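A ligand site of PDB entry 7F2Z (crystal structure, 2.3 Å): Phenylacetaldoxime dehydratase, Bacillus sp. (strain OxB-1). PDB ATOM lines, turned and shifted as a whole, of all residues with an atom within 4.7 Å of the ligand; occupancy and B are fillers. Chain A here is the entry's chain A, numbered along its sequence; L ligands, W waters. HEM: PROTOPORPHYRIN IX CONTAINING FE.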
ATOM      1  N   LEU A 128     -24.833  -8.265 -33.036  1.00  0.00           N
ATOM      2  CA  LEU A 128     -24.875  -7.448 -31.825  1.00  0.00           C
ATOM      3  C   LEU A 128     -23.453  -7.022 -31.497  1.00  0.00           C
ATOM      4  O   LEU A 128     -22.521  -7.814 -31.662  1.00  0.00           O
ATOM      5  CB  LEU A 128     -25.503  -8.198 -30.642  1.00  0.00           C
ATOM      6  CG  LEU A 128     -25.943  -7.295 -29.461  1.00  0.00           C
ATOM      7  CD1 LEU A 128     -27.012  -6.347 -29.960  1.00  0.00           C
ATOM      8  CD2 LEU A 128     -26.413  -8.069 -28.219  1.00  0.00           C
ATOM      9  N   HIS A 150     -31.984  -6.069 -27.025  1.00  0.00           N
ATOM     10  CA  HIS A 150     -30.884  -6.835 -26.465  1.00  0.00           C
ATOM     11  C   HIS A 150     -31.011  -6.812 -24.952  1.00  0.00           C
ATOM     12  O   HIS A 150     -31.842  -6.095 -24.399  1.00  0.00           O
ATOM     13  CB  HIS A 150     -29.535  -6.283 -26.920  1.00  0.00           C
ATOM     14  CG  HIS A 150     -29.067  -5.111 -26.127  1.00  0.00           C
ATOM     15  ND1 HIS A 150     -28.105  -5.213 -25.146  1.00  0.00           N
ATOM     16  CD2 HIS A 150     -29.431  -3.803 -26.153  1.00  0.00           C
ATOM     17  CE1 HIS A 150     -27.896  -4.031 -24.610  1.00  0.00           C
ATOM     18  NE2 HIS A 150     -28.692  -3.156 -25.201  1.00  0.00           N
ATOM     19  N   GLU A 151     -30.185  -7.625 -24.288  1.00  0.00           N
ATOM     20  CA  GLU A 151     -30.101  -7.702 -22.814  1.00  0.00           C
ATOM     21  C   GLU A 151     -31.352  -8.354 -22.222  1.00  0.00           C
ATOM     22  O   GLU A 151     -31.848  -7.963 -21.162  1.00  0.00           O
ATOM     23  CB  GLU A 151     -29.837  -6.332 -22.188  1.00  0.00           C
ATOM     24  CG  GLU A 151     -29.126  -6.369 -20.846  1.00  0.00           C
ATOM     25  CD  GLU A 151     -28.938  -4.996 -20.222  1.00  0.00           C
ATOM     26  OE1 GLU A 151     -29.643  -4.665 -19.229  1.00  0.00           O
ATOM     27  OE2 GLU A 151     -28.072  -4.242 -20.729  1.00  0.00           O
ATOM     28  N   TYR A 152     -31.891  -9.335 -22.942  1.00  0.00           N
ATOM     29  CA  TYR A 152     -32.919 -10.229 -22.419  1.00  0.00           C
ATOM     30  C   TYR A 152     -32.847 -11.526 -23.202  1.00  0.00           C
ATOM     31  O   TYR A 152     -32.331 -11.577 -24.325  1.00  0.00           O
ATOM     32  CB  TYR A 152     -34.323  -9.614 -22.509  1.00  0.00           C
ATOM     33  CG  TYR A 152     -34.855  -9.356 -23.915  1.00  0.00           C
ATOM     34  CD1 TYR A 152     -34.614  -8.142 -24.565  1.00  0.00           C
ATOM     35  CD2 TYR A 152     -35.616 -10.319 -24.594  1.00  0.00           C
ATOM     36  CE1 TYR A 152     -35.128  -7.892 -25.828  1.00  0.00           C
ATOM     37  CE2 TYR A 152     -36.108 -10.078 -25.862  1.00  0.00           C
ATOM     38  CZ  TYR A 152     -35.870  -8.861 -26.475  1.00  0.00           C
ATOM     39  OH  TYR A 152     -36.357  -8.607 -27.747  1.00  0.00           O
ATOM     40  N   TRP A 153     -33.346 -12.588 -22.586  1.00  0.00           N
ATOM     41  CA  TRP A 153     -33.287 -13.912 -23.191  1.00  0.00           C
ATOM     42  C   TRP A 153     -34.349 -14.016 -24.269  1.00  0.00           C
ATOM     43  O   TRP A 153     -35.542 -13.866 -23.990  1.00  0.00           O
ATOM     44  CB  TRP A 153     -33.475 -14.981 -22.114  1.00  0.00           C
ATOM     45  CG  TRP A 153     -32.326 -15.236 -21.114  1.00  0.00           C
ATOM     46  CD1 TRP A 153     -32.455 -15.854 -19.909  1.00  0.00           C
ATOM     47  CD2 TRP A 153     -30.922 -14.931 -21.257  1.00  0.00           C
ATOM     48  NE1 TRP A 153     -31.236 -15.943 -19.284  1.00  0.00           N
ATOM     49  CE2 TRP A 153     -30.280 -15.396 -20.087  1.00  0.00           C
ATOM     50  CE3 TRP A 153     -30.150 -14.305 -22.241  1.00  0.00           C
ATOM     51  CZ2 TRP A 153     -28.911 -15.253 -19.884  1.00  0.00           C
ATOM     52  CZ3 TRP A 153     -28.785 -14.183 -22.039  1.00  0.00           C
ATOM     53  CH2 TRP A 153     -28.179 -14.659 -20.869  1.00  0.00           C
ATOM     54  N   GLY A 154     -33.924 -14.256 -25.500  1.00  0.00           N
ATOM     55  CA  GLY A 154     -34.799 -14.176 -26.657  1.00  0.00           C
ATOM     56  C   GLY A 154     -34.496 -13.005 -27.570  1.00  0.00           C
ATOM     57  O   GLY A 154     -35.138 -12.869 -28.613  1.00  0.00           O
ATOM     58  N   ALA A 155     -33.524 -12.169 -27.219  1.00  0.00           N
ATOM     59  CA  ALA A 155     -33.301 -10.948 -27.987  1.00  0.00           C
ATOM     60  C   ALA A 155     -32.625 -11.260 -29.309  1.00  0.00           C
ATOM     61  O   ALA A 155     -33.001 -10.707 -30.342  1.00  0.00           O
ATOM     62  CB  ALA A 155     -32.472  -9.953 -27.181  1.00  0.00           C
ATOM     63  N   MET A 156     -31.615 -12.137 -29.278  1.00  0.00           N
ATOM     64  CA  MET A 156     -31.019 -12.678 -30.487  1.00  0.00           C
ATOM     65  C   MET A 156     -32.084 -13.164 -31.465  1.00  0.00           C
ATOM     66  O   MET A 156     -32.043 -12.835 -32.655  1.00  0.00           O
ATOM     67  CB  MET A 156     -30.052 -13.828 -30.134  1.00  0.00           C
ATOM     68  CG  MET A 156     -29.777 -14.754 -31.303  1.00  0.00           C
ATOM     69  SD  MET A 156     -28.631 -16.119 -31.004  1.00  0.00           S
ATOM     70  CE  MET A 156     -29.598 -17.083 -29.825  1.00  0.00           C
ATOM     71  N   ARG A 159     -33.969 -10.209 -32.826  1.00  0.00           N
ATOM     72  CA  ARG A 159     -33.211  -9.407 -33.776  1.00  0.00           C
ATOM     73  C   ARG A 159     -33.186 -10.030 -35.157  1.00  0.00           C
ATOM     74  O   ARG A 159     -32.976  -9.307 -36.140  1.00  0.00           O
ATOM     75  CB  ARG A 159     -31.755  -9.168 -33.291  1.00  0.00           C
ATOM     76  CG  ARG A 159     -31.623  -8.026 -32.231  1.00  0.00           C
ATOM     77  CD  ARG A 159     -30.159  -7.613 -31.987  1.00  0.00           C
ATOM     78  NE  ARG A 159     -29.312  -8.775 -31.754  1.00  0.00           N
ATOM     79  CZ  ARG A 159     -29.223  -9.407 -30.578  1.00  0.00           C
ATOM     80  NH1 ARG A 159     -29.915  -8.964 -29.520  1.00  0.00           N
ATOM     81  NH2 ARG A 159     -28.441 -10.474 -30.454  1.00  0.00           N
ATOM     82  N   ILE A 200     -22.938 -19.294 -35.120  1.00  0.00           N
ATOM     83  CA  ILE A 200     -22.597 -18.091 -34.377  1.00  0.00           C
ATOM     84  C   ILE A 200     -21.093 -17.877 -34.465  1.00  0.00           C
ATOM     85  O   ILE A 200     -20.315 -18.826 -34.370  1.00  0.00           O
ATOM     86  CB  ILE A 200     -23.035 -18.150 -32.885  1.00  0.00           C
ATOM     87  CG1 ILE A 200     -22.590 -16.883 -32.141  1.00  0.00           C
ATOM     88  CG2 ILE A 200     -22.495 -19.412 -32.170  1.00  0.00           C
ATOM     89  CD1 ILE A 200     -23.189 -16.735 -30.727  1.00  0.00           C
ATOM     90  N   THR A 202     -18.930 -15.469 -32.095  1.00  0.00           N
ATOM     91  CA  THR A 202     -19.031 -14.576 -30.938  1.00  0.00           C
ATOM     92  C   THR A 202     -17.611 -14.235 -30.493  1.00  0.00           C
ATOM     93  O   THR A 202     -16.775 -15.120 -30.310  1.00  0.00           O
ATOM     94  CB  THR A 202     -19.866 -15.230 -29.815  1.00  0.00           C
ATOM     95  OG1 THR A 202     -20.072 -14.304 -28.734  1.00  0.00           O
ATOM     96  CG2 THR A 202     -19.240 -16.541 -29.290  1.00  0.00           C
ATOM     97  N   GLN A 204     -14.358 -11.669 -28.782  1.00  0.00           N
ATOM     98  CA  GLN A 204     -13.774 -10.962 -27.658  1.00  0.00           C
ATOM     99  C   GLN A 204     -12.607 -10.131 -28.177  1.00  0.00           C
ATOM    100  O   GLN A 204     -11.715 -10.672 -28.831  1.00  0.00           O
ATOM    101  CB  GLN A 204     -13.285 -11.937 -26.585  1.00  0.00           C
ATOM    102  CG  GLN A 204     -14.295 -12.983 -26.118  1.00  0.00           C
ATOM    103  CD  GLN A 204     -14.592 -14.029 -27.179  1.00  0.00           C
ATOM    104  OE1 GLN A 204     -13.691 -14.503 -27.893  1.00  0.00           O
ATOM    105  NE2 GLN A 204     -15.881 -14.387 -27.301  1.00  0.00           N
ATOM    106  N   VAL A 221     -12.083 -13.769 -16.874  1.00  0.00           N
ATOM    107  CA  VAL A 221     -13.079 -14.108 -17.877  1.00  0.00           C
ATOM    108  C   VAL A 221     -12.576 -15.180 -18.850  1.00  0.00           C
ATOM    109  O   VAL A 221     -13.274 -16.160 -19.119  1.00  0.00           O
ATOM    110  CB  VAL A 221     -13.522 -12.846 -18.640  1.00  0.00           C
ATOM    111  CG1 VAL A 221     -14.591 -13.213 -19.671  1.00  0.00           C
ATOM    112  CG2 VAL A 221     -14.052 -11.813 -17.676  1.00  0.00           C
ATOM    113  N   LEU A 225     -14.384 -18.791 -20.561  1.00  0.00           N
ATOM    114  CA  LEU A 225     -14.663 -18.945 -21.996  1.00  0.00           C
ATOM    115  C   LEU A 225     -14.028 -20.216 -22.542  1.00  0.00           C
ATOM    116  O   LEU A 225     -14.654 -20.955 -23.307  1.00  0.00           O
ATOM    117  CB  LEU A 225     -14.167 -17.724 -22.780  1.00  0.00           C
ATOM    118  CG  LEU A 225     -14.181 -17.865 -24.318  1.00  0.00           C
ATOM    119  CD1 LEU A 225     -15.596 -17.976 -24.852  1.00  0.00           C
ATOM    120  CD2 LEU A 225     -13.457 -16.694 -24.958  1.00  0.00           C
ATOM    121  N   ALA A 228     -15.976 -23.105 -21.288  1.00  0.00           N
ATOM    122  CA  ALA A 228     -17.190 -23.174 -22.105  1.00  0.00           C
ATOM    123  C   ALA A 228     -16.936 -23.913 -23.411  1.00  0.00           C
ATOM    124  O   ALA A 228     -17.659 -24.851 -23.757  1.00  0.00           O
ATOM    125  CB  ALA A 228     -17.718 -21.763 -22.400  1.00  0.00           C
ATOM    126  N   LEU A 232     -18.303 -27.533 -24.792  1.00  0.00           N
ATOM    127  CA  LEU A 232     -19.093 -27.660 -26.012  1.00  0.00           C
ATOM    128  C   LEU A 232     -18.482 -28.675 -26.973  1.00  0.00           C
ATOM    129  O   LEU A 232     -19.212 -29.464 -27.595  1.00  0.00           O
ATOM    130  CB  LEU A 232     -19.250 -26.298 -26.683  1.00  0.00           C
ATOM    131  CG  LEU A 232     -20.192 -25.323 -25.969  1.00  0.00           C
ATOM    132  CD1 LEU A 232     -19.947 -23.887 -26.439  1.00  0.00           C
ATOM    133  CD2 LEU A 232     -21.642 -25.727 -26.187  1.00  0.00           C
ATOM    134  N   VAL A 262     -15.223 -17.359 -30.734  1.00  0.00           N
ATOM    135  CA  VAL A 262     -15.714 -18.727 -30.820  1.00  0.00           C
ATOM    136  C   VAL A 262     -16.594 -18.834 -32.052  1.00  0.00           C
ATOM    137  O   VAL A 262     -17.481 -17.995 -32.274  1.00  0.00           O
ATOM    138  CB  VAL A 262     -16.496 -19.126 -29.561  1.00  0.00           C
ATOM    139  CG1 VAL A 262     -17.252 -20.453 -29.816  1.00  0.00           C
ATOM    140  CG2 VAL A 262     -15.549 -19.261 -28.369  1.00  0.00           C
ATOM    141  N   TYR A 266     -24.731 -25.123 -34.299  1.00  0.00           N
ATOM    142  CA  TYR A 266     -25.650 -25.776 -33.406  1.00  0.00           C
ATOM    143  C   TYR A 266     -26.781 -26.350 -34.217  1.00  0.00           C
ATOM    144  O   TYR A 266     -27.106 -25.850 -35.301  1.00  0.00           O
ATOM    145  CB  TYR A 266     -26.214 -24.795 -32.363  1.00  0.00           C
ATOM    146  CG  TYR A 266     -25.177 -24.378 -31.360  1.00  0.00           C
ATOM    147  CD1 TYR A 266     -24.194 -23.432 -31.681  1.00  0.00           C
ATOM    148  CD2 TYR A 266     -25.159 -24.931 -30.094  1.00  0.00           C
ATOM    149  CE1 TYR A 266     -23.222 -23.061 -30.736  1.00  0.00           C
ATOM    150  CE2 TYR A 266     -24.219 -24.566 -29.157  1.00  0.00           C
ATOM    151  CZ  TYR A 266     -23.259 -23.629 -29.481  1.00  0.00           C
ATOM    152  OH  TYR A 266     -22.345 -23.296 -28.525  1.00  0.00           O
ATOM    153  N   LEU A 272     -28.731 -23.413 -29.135  1.00  0.00           N
ATOM    154  CA  LEU A 272     -27.829 -22.352 -28.691  1.00  0.00           C
ATOM    155  C   LEU A 272     -28.437 -21.553 -27.541  1.00  0.00           C
ATOM    156  O   LEU A 272     -27.768 -21.303 -26.522  1.00  0.00           O
ATOM    157  CB  LEU A 272     -27.480 -21.444 -29.879  1.00  0.00           C
ATOM    158  CG  LEU A 272     -26.674 -20.183 -29.569  1.00  0.00           C
ATOM    159  CD1 LEU A 272     -25.335 -20.500 -28.886  1.00  0.00           C
ATOM    160  CD2 LEU A 272     -26.433 -19.351 -30.840  1.00  0.00           C
ATOM    161  N   GLU A 273     -29.715 -21.189 -27.658  1.00  0.00           N
ATOM    162  CA  GLU A 273     -30.413 -20.479 -26.589  1.00  0.00           C
ATOM    163  C   GLU A 273     -30.424 -21.267 -25.285  1.00  0.00           C
ATOM    164  O   GLU A 273     -30.188 -20.705 -24.209  1.00  0.00           O
ATOM    165  CB  GLU A 273     -31.855 -20.178 -27.024  1.00  0.00           C
ATOM    166  CG  GLU A 273     -32.007 -19.035 -28.006  1.00  0.00           C
ATOM    167  CD  GLU A 273     -33.436 -18.907 -28.498  1.00  0.00           C
ATOM    168  OE1 GLU A 273     -34.150 -19.938 -28.565  1.00  0.00           O
ATOM    169  OE2 GLU A 273     -33.843 -17.768 -28.821  1.00  0.00           O
ATOM    170  N   TRP A 275     -28.389 -23.649 -24.220  1.00  0.00           N
ATOM    171  CA  TRP A 275     -27.049 -23.639 -23.641  1.00  0.00           C
ATOM    172  C   TRP A 275     -26.728 -22.285 -23.031  1.00  0.00           C
ATOM    173  O   TRP A 275     -26.298 -22.193 -21.871  1.00  0.00           O
ATOM    174  CB  TRP A 275     -26.002 -24.018 -24.689  1.00  0.00           C
ATOM    175  CG  TRP A 275     -24.632 -24.028 -24.117  1.00  0.00           C
ATOM    176  CD1 TRP A 275     -24.045 -25.042 -23.422  1.00  0.00           C
ATOM    177  CD2 TRP A 275     -23.685 -22.944 -24.099  1.00  0.00           C
ATOM    178  NE1 TRP A 275     -22.786 -24.682 -23.004  1.00  0.00           N
ATOM    179  CE2 TRP A 275     -22.540 -23.399 -23.403  1.00  0.00           C
ATOM    180  CE3 TRP A 275     -23.685 -21.644 -24.620  1.00  0.00           C
ATOM    181  CZ2 TRP A 275     -21.409 -22.591 -23.219  1.00  0.00           C
ATOM    182  CZ3 TRP A 275     -22.563 -20.844 -24.444  1.00  0.00           C
ATOM    183  CH2 TRP A 275     -21.440 -21.326 -23.737  1.00  0.00           C
ATOM    184  N   THR A 276     -26.940 -21.202 -23.790  1.00  0.00           N
ATOM    185  CA  THR A 276     -26.578 -19.869 -23.293  1.00  0.00           C
ATOM    186  C   THR A 276     -27.340 -19.521 -22.010  1.00  0.00           C
ATOM    187  O   THR A 276     -26.742 -19.079 -21.027  1.00  0.00           O
ATOM    188  CB  THR A 276     -26.851 -18.813 -24.359  1.00  0.00           C
ATOM    189  OG1 THR A 276     -26.066 -19.100 -25.523  1.00  0.00           O
ATOM    190  CG2 THR A 276     -26.513 -17.422 -23.820  1.00  0.00           C
ATOM    191  N   HIS A 277     -28.663 -19.720 -22.005  1.00  0.00           N
ATOM    192  CA  HIS A 277     -29.515 -19.243 -20.915  1.00  0.00           C
ATOM    193  C   HIS A 277     -29.390 -20.108 -19.667  1.00  0.00           C
ATOM    194  O   HIS A 277     -29.467 -19.590 -18.554  1.00  0.00           O
ATOM    195  CB  HIS A 277     -30.983 -19.217 -21.345  1.00  0.00           C
ATOM    196  CG  HIS A 277     -31.253 -18.355 -22.535  1.00  0.00           C
ATOM    197  ND1 HIS A 277     -32.471 -18.360 -23.196  1.00  0.00           N
ATOM    198  CD2 HIS A 277     -30.476 -17.465 -23.206  1.00  0.00           C
ATOM    199  CE1 HIS A 277     -32.417 -17.522 -24.215  1.00  0.00           C
ATOM    200  NE2 HIS A 277     -31.220 -16.968 -24.239  1.00  0.00           N
ATOM    201  N   HIS A 282     -21.814 -20.855 -19.359  1.00  0.00           N
ATOM    202  CA  HIS A 282     -22.029 -19.480 -19.794  1.00  0.00           C
ATOM    203  C   HIS A 282     -22.533 -18.597 -18.658  1.00  0.00           C
ATOM    204  O   HIS A 282     -22.147 -17.422 -18.566  1.00  0.00           O
ATOM    205  CB  HIS A 282     -23.016 -19.425 -20.962  1.00  0.00           C
ATOM    206  CG  HIS A 282     -23.170 -18.059 -21.555  1.00  0.00           C
ATOM    207  ND1 HIS A 282     -24.053 -17.126 -21.041  1.00  0.00           N
ATOM    208  CD2 HIS A 282     -22.557 -17.462 -22.601  1.00  0.00           C
ATOM    209  CE1 HIS A 282     -23.976 -16.009 -21.754  1.00  0.00           C
ATOM    210  NE2 HIS A 282     -23.067 -16.191 -22.698  1.00  0.00           N
ATOM    211  N   ILE A 285     -19.577 -17.366 -17.360  1.00  0.00           N
ATOM    212  CA  ILE A 285     -18.959 -16.300 -18.160  1.00  0.00           C
ATOM    213  C   ILE A 285     -19.644 -14.966 -17.919  1.00  0.00           C
ATOM    214  O   ILE A 285     -18.989 -13.928 -17.756  1.00  0.00           O
ATOM    215  CB  ILE A 285     -19.009 -16.647 -19.649  1.00  0.00           C
ATOM    216  CG1 ILE A 285     -18.285 -17.954 -19.943  1.00  0.00           C
ATOM    217  CG2 ILE A 285     -18.421 -15.514 -20.443  1.00  0.00           C
ATOM    218  CD1 ILE A 285     -18.411 -18.376 -21.373  1.00  0.00           C
ATOM    219  N   TYR A 286     -20.970 -14.962 -17.974  1.00  0.00           N
ATOM    220  CA  TYR A 286     -21.755 -13.754 -17.726  1.00  0.00           C
ATOM    221  C   TYR A 286     -21.531 -13.233 -16.316  1.00  0.00           C
ATOM    222  O   TYR A 286     -21.631 -12.025 -16.067  1.00  0.00           O
ATOM    223  CB  TYR A 286     -23.227 -14.073 -17.975  1.00  0.00           C
ATOM    224  CG  TYR A 286     -24.156 -12.933 -18.375  1.00  0.00           C
ATOM    225  CD1 TYR A 286     -24.239 -11.770 -17.618  1.00  0.00           C
ATOM    226  CD2 TYR A 286     -24.991 -13.053 -19.478  1.00  0.00           C
ATOM    227  CE1 TYR A 286     -25.115 -10.754 -17.979  1.00  0.00           C
ATOM    228  CE2 TYR A 286     -25.854 -12.045 -19.849  1.00  0.00           C
ATOM    229  CZ  TYR A 286     -25.907 -10.902 -19.098  1.00  0.00           C
ATOM    230  OH  TYR A 286     -26.792  -9.911 -19.477  1.00  0.00           O
ATOM    231  N   PHE A 289     -18.061 -11.697 -16.107  1.00  0.00           N
ATOM    232  CA  PHE A 289     -18.120 -10.464 -16.881  1.00  0.00           C
ATOM    233  C   PHE A 289     -18.712  -9.330 -16.060  1.00  0.00           C
ATOM    234  O   PHE A 289     -18.270  -8.181 -16.177  1.00  0.00           O
ATOM    235  CB  PHE A 289     -18.939 -10.664 -18.155  1.00  0.00           C
ATOM    236  CG  PHE A 289     -19.015  -9.435 -19.026  1.00  0.00           C
ATOM    237  CD1 PHE A 289     -17.861  -8.787 -19.436  1.00  0.00           C
ATOM    238  CD2 PHE A 289     -20.239  -8.935 -19.442  1.00  0.00           C
ATOM    239  CE1 PHE A 289     -17.922  -7.670 -20.247  1.00  0.00           C
ATOM    240  CE2 PHE A 289     -20.296  -7.814 -20.261  1.00  0.00           C
ATOM    241  CZ  PHE A 289     -19.138  -7.182 -20.663  1.00  0.00           C
ATOM    242  N   LEU A 304     -17.186  -6.670 -27.206  1.00  0.00           N
ATOM    243  CA  LEU A 304     -17.780  -7.955 -27.590  1.00  0.00           C
ATOM    244  C   LEU A 304     -18.677  -7.743 -28.802  1.00  0.00           C
ATOM    245  O   LEU A 304     -19.123  -6.631 -29.072  1.00  0.00           O
ATOM    246  CB  LEU A 304     -18.578  -8.582 -26.433  1.00  0.00           C
ATOM    247  CG  LEU A 304     -17.878  -8.586 -25.068  1.00  0.00           C
ATOM    248  CD1 LEU A 304     -18.809  -9.017 -23.954  1.00  0.00           C
ATOM    249  CD2 LEU A 304     -16.648  -9.498 -25.112  1.00  0.00           C
ATOM    250  N   HIS A 306     -21.263 -10.368 -31.821  1.00  0.00           N
ATOM    251  CA  HIS A 306     -21.513 -11.662 -32.462  1.00  0.00           C
ATOM    252  C   HIS A 306     -22.332 -11.491 -33.729  1.00  0.00           C
ATOM    253  O   HIS A 306     -23.041 -10.496 -33.913  1.00  0.00           O
ATOM    254  CB  HIS A 306     -22.124 -12.670 -31.454  1.00  0.00           C
ATOM    255  CG  HIS A 306     -23.601 -12.568 -31.238  1.00  0.00           C
ATOM    256  ND1 HIS A 306     -24.190 -13.022 -30.080  1.00  0.00           N
ATOM    257  CD2 HIS A 306     -24.620 -12.159 -32.027  1.00  0.00           C
ATOM    258  CE1 HIS A 306     -25.506 -12.873 -30.153  1.00  0.00           C
ATOM    259  NE2 HIS A 306     -25.785 -12.336 -31.330  1.00  0.00           N
HETATM  260  CHA HEM L   1     -25.523 -13.056 -24.891  1.00  0.00           C
HETATM  261  CHB HEM L   1     -23.592 -17.070 -26.769  1.00  0.00           C
HETATM  262  CHC HEM L   1     -19.338 -16.078 -24.721  1.00  0.00           C
HETATM  263  CHD HEM L   1     -21.378 -12.327 -22.514  1.00  0.00           C
HETATM  264  C1A HEM L   1     -25.335 -14.193 -25.618  1.00  0.00           C
HETATM  265  C2A HEM L   1     -26.313 -14.745 -26.522  1.00  0.00           C
HETATM  266  C3A HEM L   1     -25.778 -15.853 -27.049  1.00  0.00           C
HETATM  267  C4A HEM L   1     -24.454 -16.026 -26.486  1.00  0.00           C
HETATM  268  CMA HEM L   1     -26.443 -16.815 -28.074  1.00  0.00           C
HETATM  269  CAA HEM L   1     -27.701 -14.099 -26.799  1.00  0.00           C
HETATM  270  CBA HEM L   1     -28.788 -14.805 -25.986  1.00  0.00           C
HETATM  271  CGA HEM L   1     -30.161 -14.289 -26.297  1.00  0.00           C
HETATM  272  O1A HEM L   1     -31.124 -15.035 -26.012  1.00  0.00           O
HETATM  273  O2A HEM L   1     -30.320 -13.151 -26.825  1.00  0.00           O
HETATM  274  C1B HEM L   1     -22.282 -17.166 -26.373  1.00  0.00           C
HETATM  275  C2B HEM L   1     -21.359 -18.259 -26.674  1.00  0.00           C
HETATM  276  C3B HEM L   1     -20.185 -17.945 -26.100  1.00  0.00           C
HETATM  277  C4B HEM L   1     -20.350 -16.695 -25.416  1.00  0.00           C
HETATM  278  CMB HEM L   1     -21.665 -19.513 -27.536  1.00  0.00           C
HETATM  279  CAB HEM L   1     -18.852 -18.729 -26.073  1.00  0.00           C
HETATM  280  CBB HEM L   1     -18.748 -20.046 -26.289  1.00  0.00           C
HETATM  281  C1C HEM L   1     -19.496 -14.933 -24.011  1.00  0.00           C
HETATM  282  C2C HEM L   1     -18.432 -14.116 -23.459  1.00  0.00           C
HETATM  283  C3C HEM L   1     -19.015 -13.071 -22.854  1.00  0.00           C
HETATM  284  C4C HEM L   1     -20.445 -13.204 -23.009  1.00  0.00           C
HETATM  285  CMC HEM L   1     -16.919 -14.452 -23.578  1.00  0.00           C
HETATM  286  CAC HEM L   1     -18.390 -11.901 -22.066  1.00  0.00           C
HETATM  287  CBC HEM L   1     -17.082 -11.824 -21.779  1.00  0.00           C
HETATM  288  C1D HEM L   1     -22.650 -12.184 -23.002  1.00  0.00           C
HETATM  289  C2D HEM L   1     -23.534 -11.065 -22.730  1.00  0.00           C
HETATM  290  C3D HEM L   1     -24.673 -11.271 -23.379  1.00  0.00           C
HETATM  291  C4D HEM L   1     -24.562 -12.517 -24.090  1.00  0.00           C
HETATM  292  CMD HEM L   1     -23.223  -9.856 -21.826  1.00  0.00           C
HETATM  293  CAD HEM L   1     -25.900 -10.334 -23.382  1.00  0.00           C
HETATM  294  CBD HEM L   1     -25.918  -9.592 -24.725  1.00  0.00           C
HETATM  295  CGD HEM L   1     -27.144  -8.729 -24.803  1.00  0.00           C
HETATM  296  O1D HEM L   1     -28.205  -9.187 -25.304  1.00  0.00           O
HETATM  297  O2D HEM L   1     -27.082  -7.554 -24.373  1.00  0.00           O
HETATM  298  NA  HEM L   1     -24.209 -14.985 -25.605  1.00  0.00           N
HETATM  299  NB  HEM L   1     -21.639 -16.234 -25.586  1.00  0.00           N
HETATM  300  NC  HEM L   1     -20.709 -14.355 -23.746  1.00  0.00           N
HETATM  301  ND  HEM L   1     -23.309 -13.066 -23.859  1.00  0.00           N
HETATM  302 FE   HEM L   1     -22.528 -14.768 -24.563  1.00  0.00          FE
HETATM  303  O   HOH W   1     -32.669 -15.454 -28.530  1.00  0.00           O
HETATM  304  O   HOH W   2     -28.781 -10.785 -27.521  1.00  0.00           O
HETATM  305  O   HOH W   3     -29.399 -11.441 -23.969  1.00  0.00           O
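Merely in contact with the ligand: Ile 285, Thr 276, Leu 304, Trp 275, Val 221, Leu 128, Leu 225, Tyr 152, Thr 202, Leu 272, Trp 153, Tyr 286, Val 262, Gln 204, Phe 289, Tyr 266 and Ile 200. Hydrophobic or aromatic side chains that line the ligand: Leu 128, His 150, Trp 153, Ala 155, Met 156, Ile 200, Val 221, Leu 225, Val 262, Leu 272, Trp 275, His 277, His 282, Ile 285, Tyr 286, Phe 289 and Leu 304. 24 residues have an atom within 4 Å of the ligand: Leu 128, His 150, Glu 151, Tyr 152, Trp 153, Gly 154, Ala 155, Met 156, Ile 200, Thr 202, Gln 204, Val 221, Leu 225, Val 262, Tyr 266, Leu 272, Trp 275, Thr 276, His 277, His 282, Ile 285, Tyr 286, Phe 289 and Leu 304.
Water W2 lies within hydrogen-bond range of O1D of the ligand and NH1 of Arg 159. Water W3 lies within hydrogen-bond range of an oxygen (O1D) of the ligand (2.9 Å) and the backbone carbonyl oxygen of Tyr 152 (3.0 Å). Water W1 lies within hydrogen-bond range of the side-chain carboxylate of Glu 273 (2.6 Å), an oxygen (O1A) of the ligand (3.0 Å) and the backbone NH of Gly 154 (3.5 Å).
The backbone NH (N) of Gly 154 sits at hydrogen-bond distance from an oxygen (O1A) of the ligand, 3.0 Å away. O2D of the ligand is in hydrogen-bond range of ND1 of His 150 (2.7 Å). O2A of the ligand sits at hydrogen-bond distance from N of Met 156, 3.0 Å away. N of Glu 151 lies within hydrogen-bond range of O1D of the ligand, 2.7 Å away. NE2 of His 277 is in hydrogen-bond range of O1A of the ligand, at 2.6 Å. An oxygen (O2A) of the ligand sits at hydrogen-bond distance from the backbone NH (N) of Ala 155 (3.4 Å). An iron atom (FE) of the ligand is bound by a ring nitrogen (NE2) of His 282.
The backbone NH (N) of His 306 lies within hydrogen-bond range of the backbone carbonyl oxygen (O) of Leu 128 (2.9 Å). The backbone carbonyl oxygen (O) of Thr 202 sits at hydrogen-bond distance from the side-chain amide nitrogen (NE2) of Gln 204. A ring nitrogen (ND1) of His 282 is in hydrogen-bond range of the backbone carbonyl oxygen (O) of Thr 276 (3.3 Å). O of Leu 272 sits at hydrogen-bond distance from OG1 of Thr 276, 3.0 Å away. O of Thr 202 sits at hydrogen-bond distance from N of Val 262, at 2.8 Å. A ring nitrogen (ND1) of His 277 sits close to the backbone carbonyl oxygen of Glu 273 (3.4 Å).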
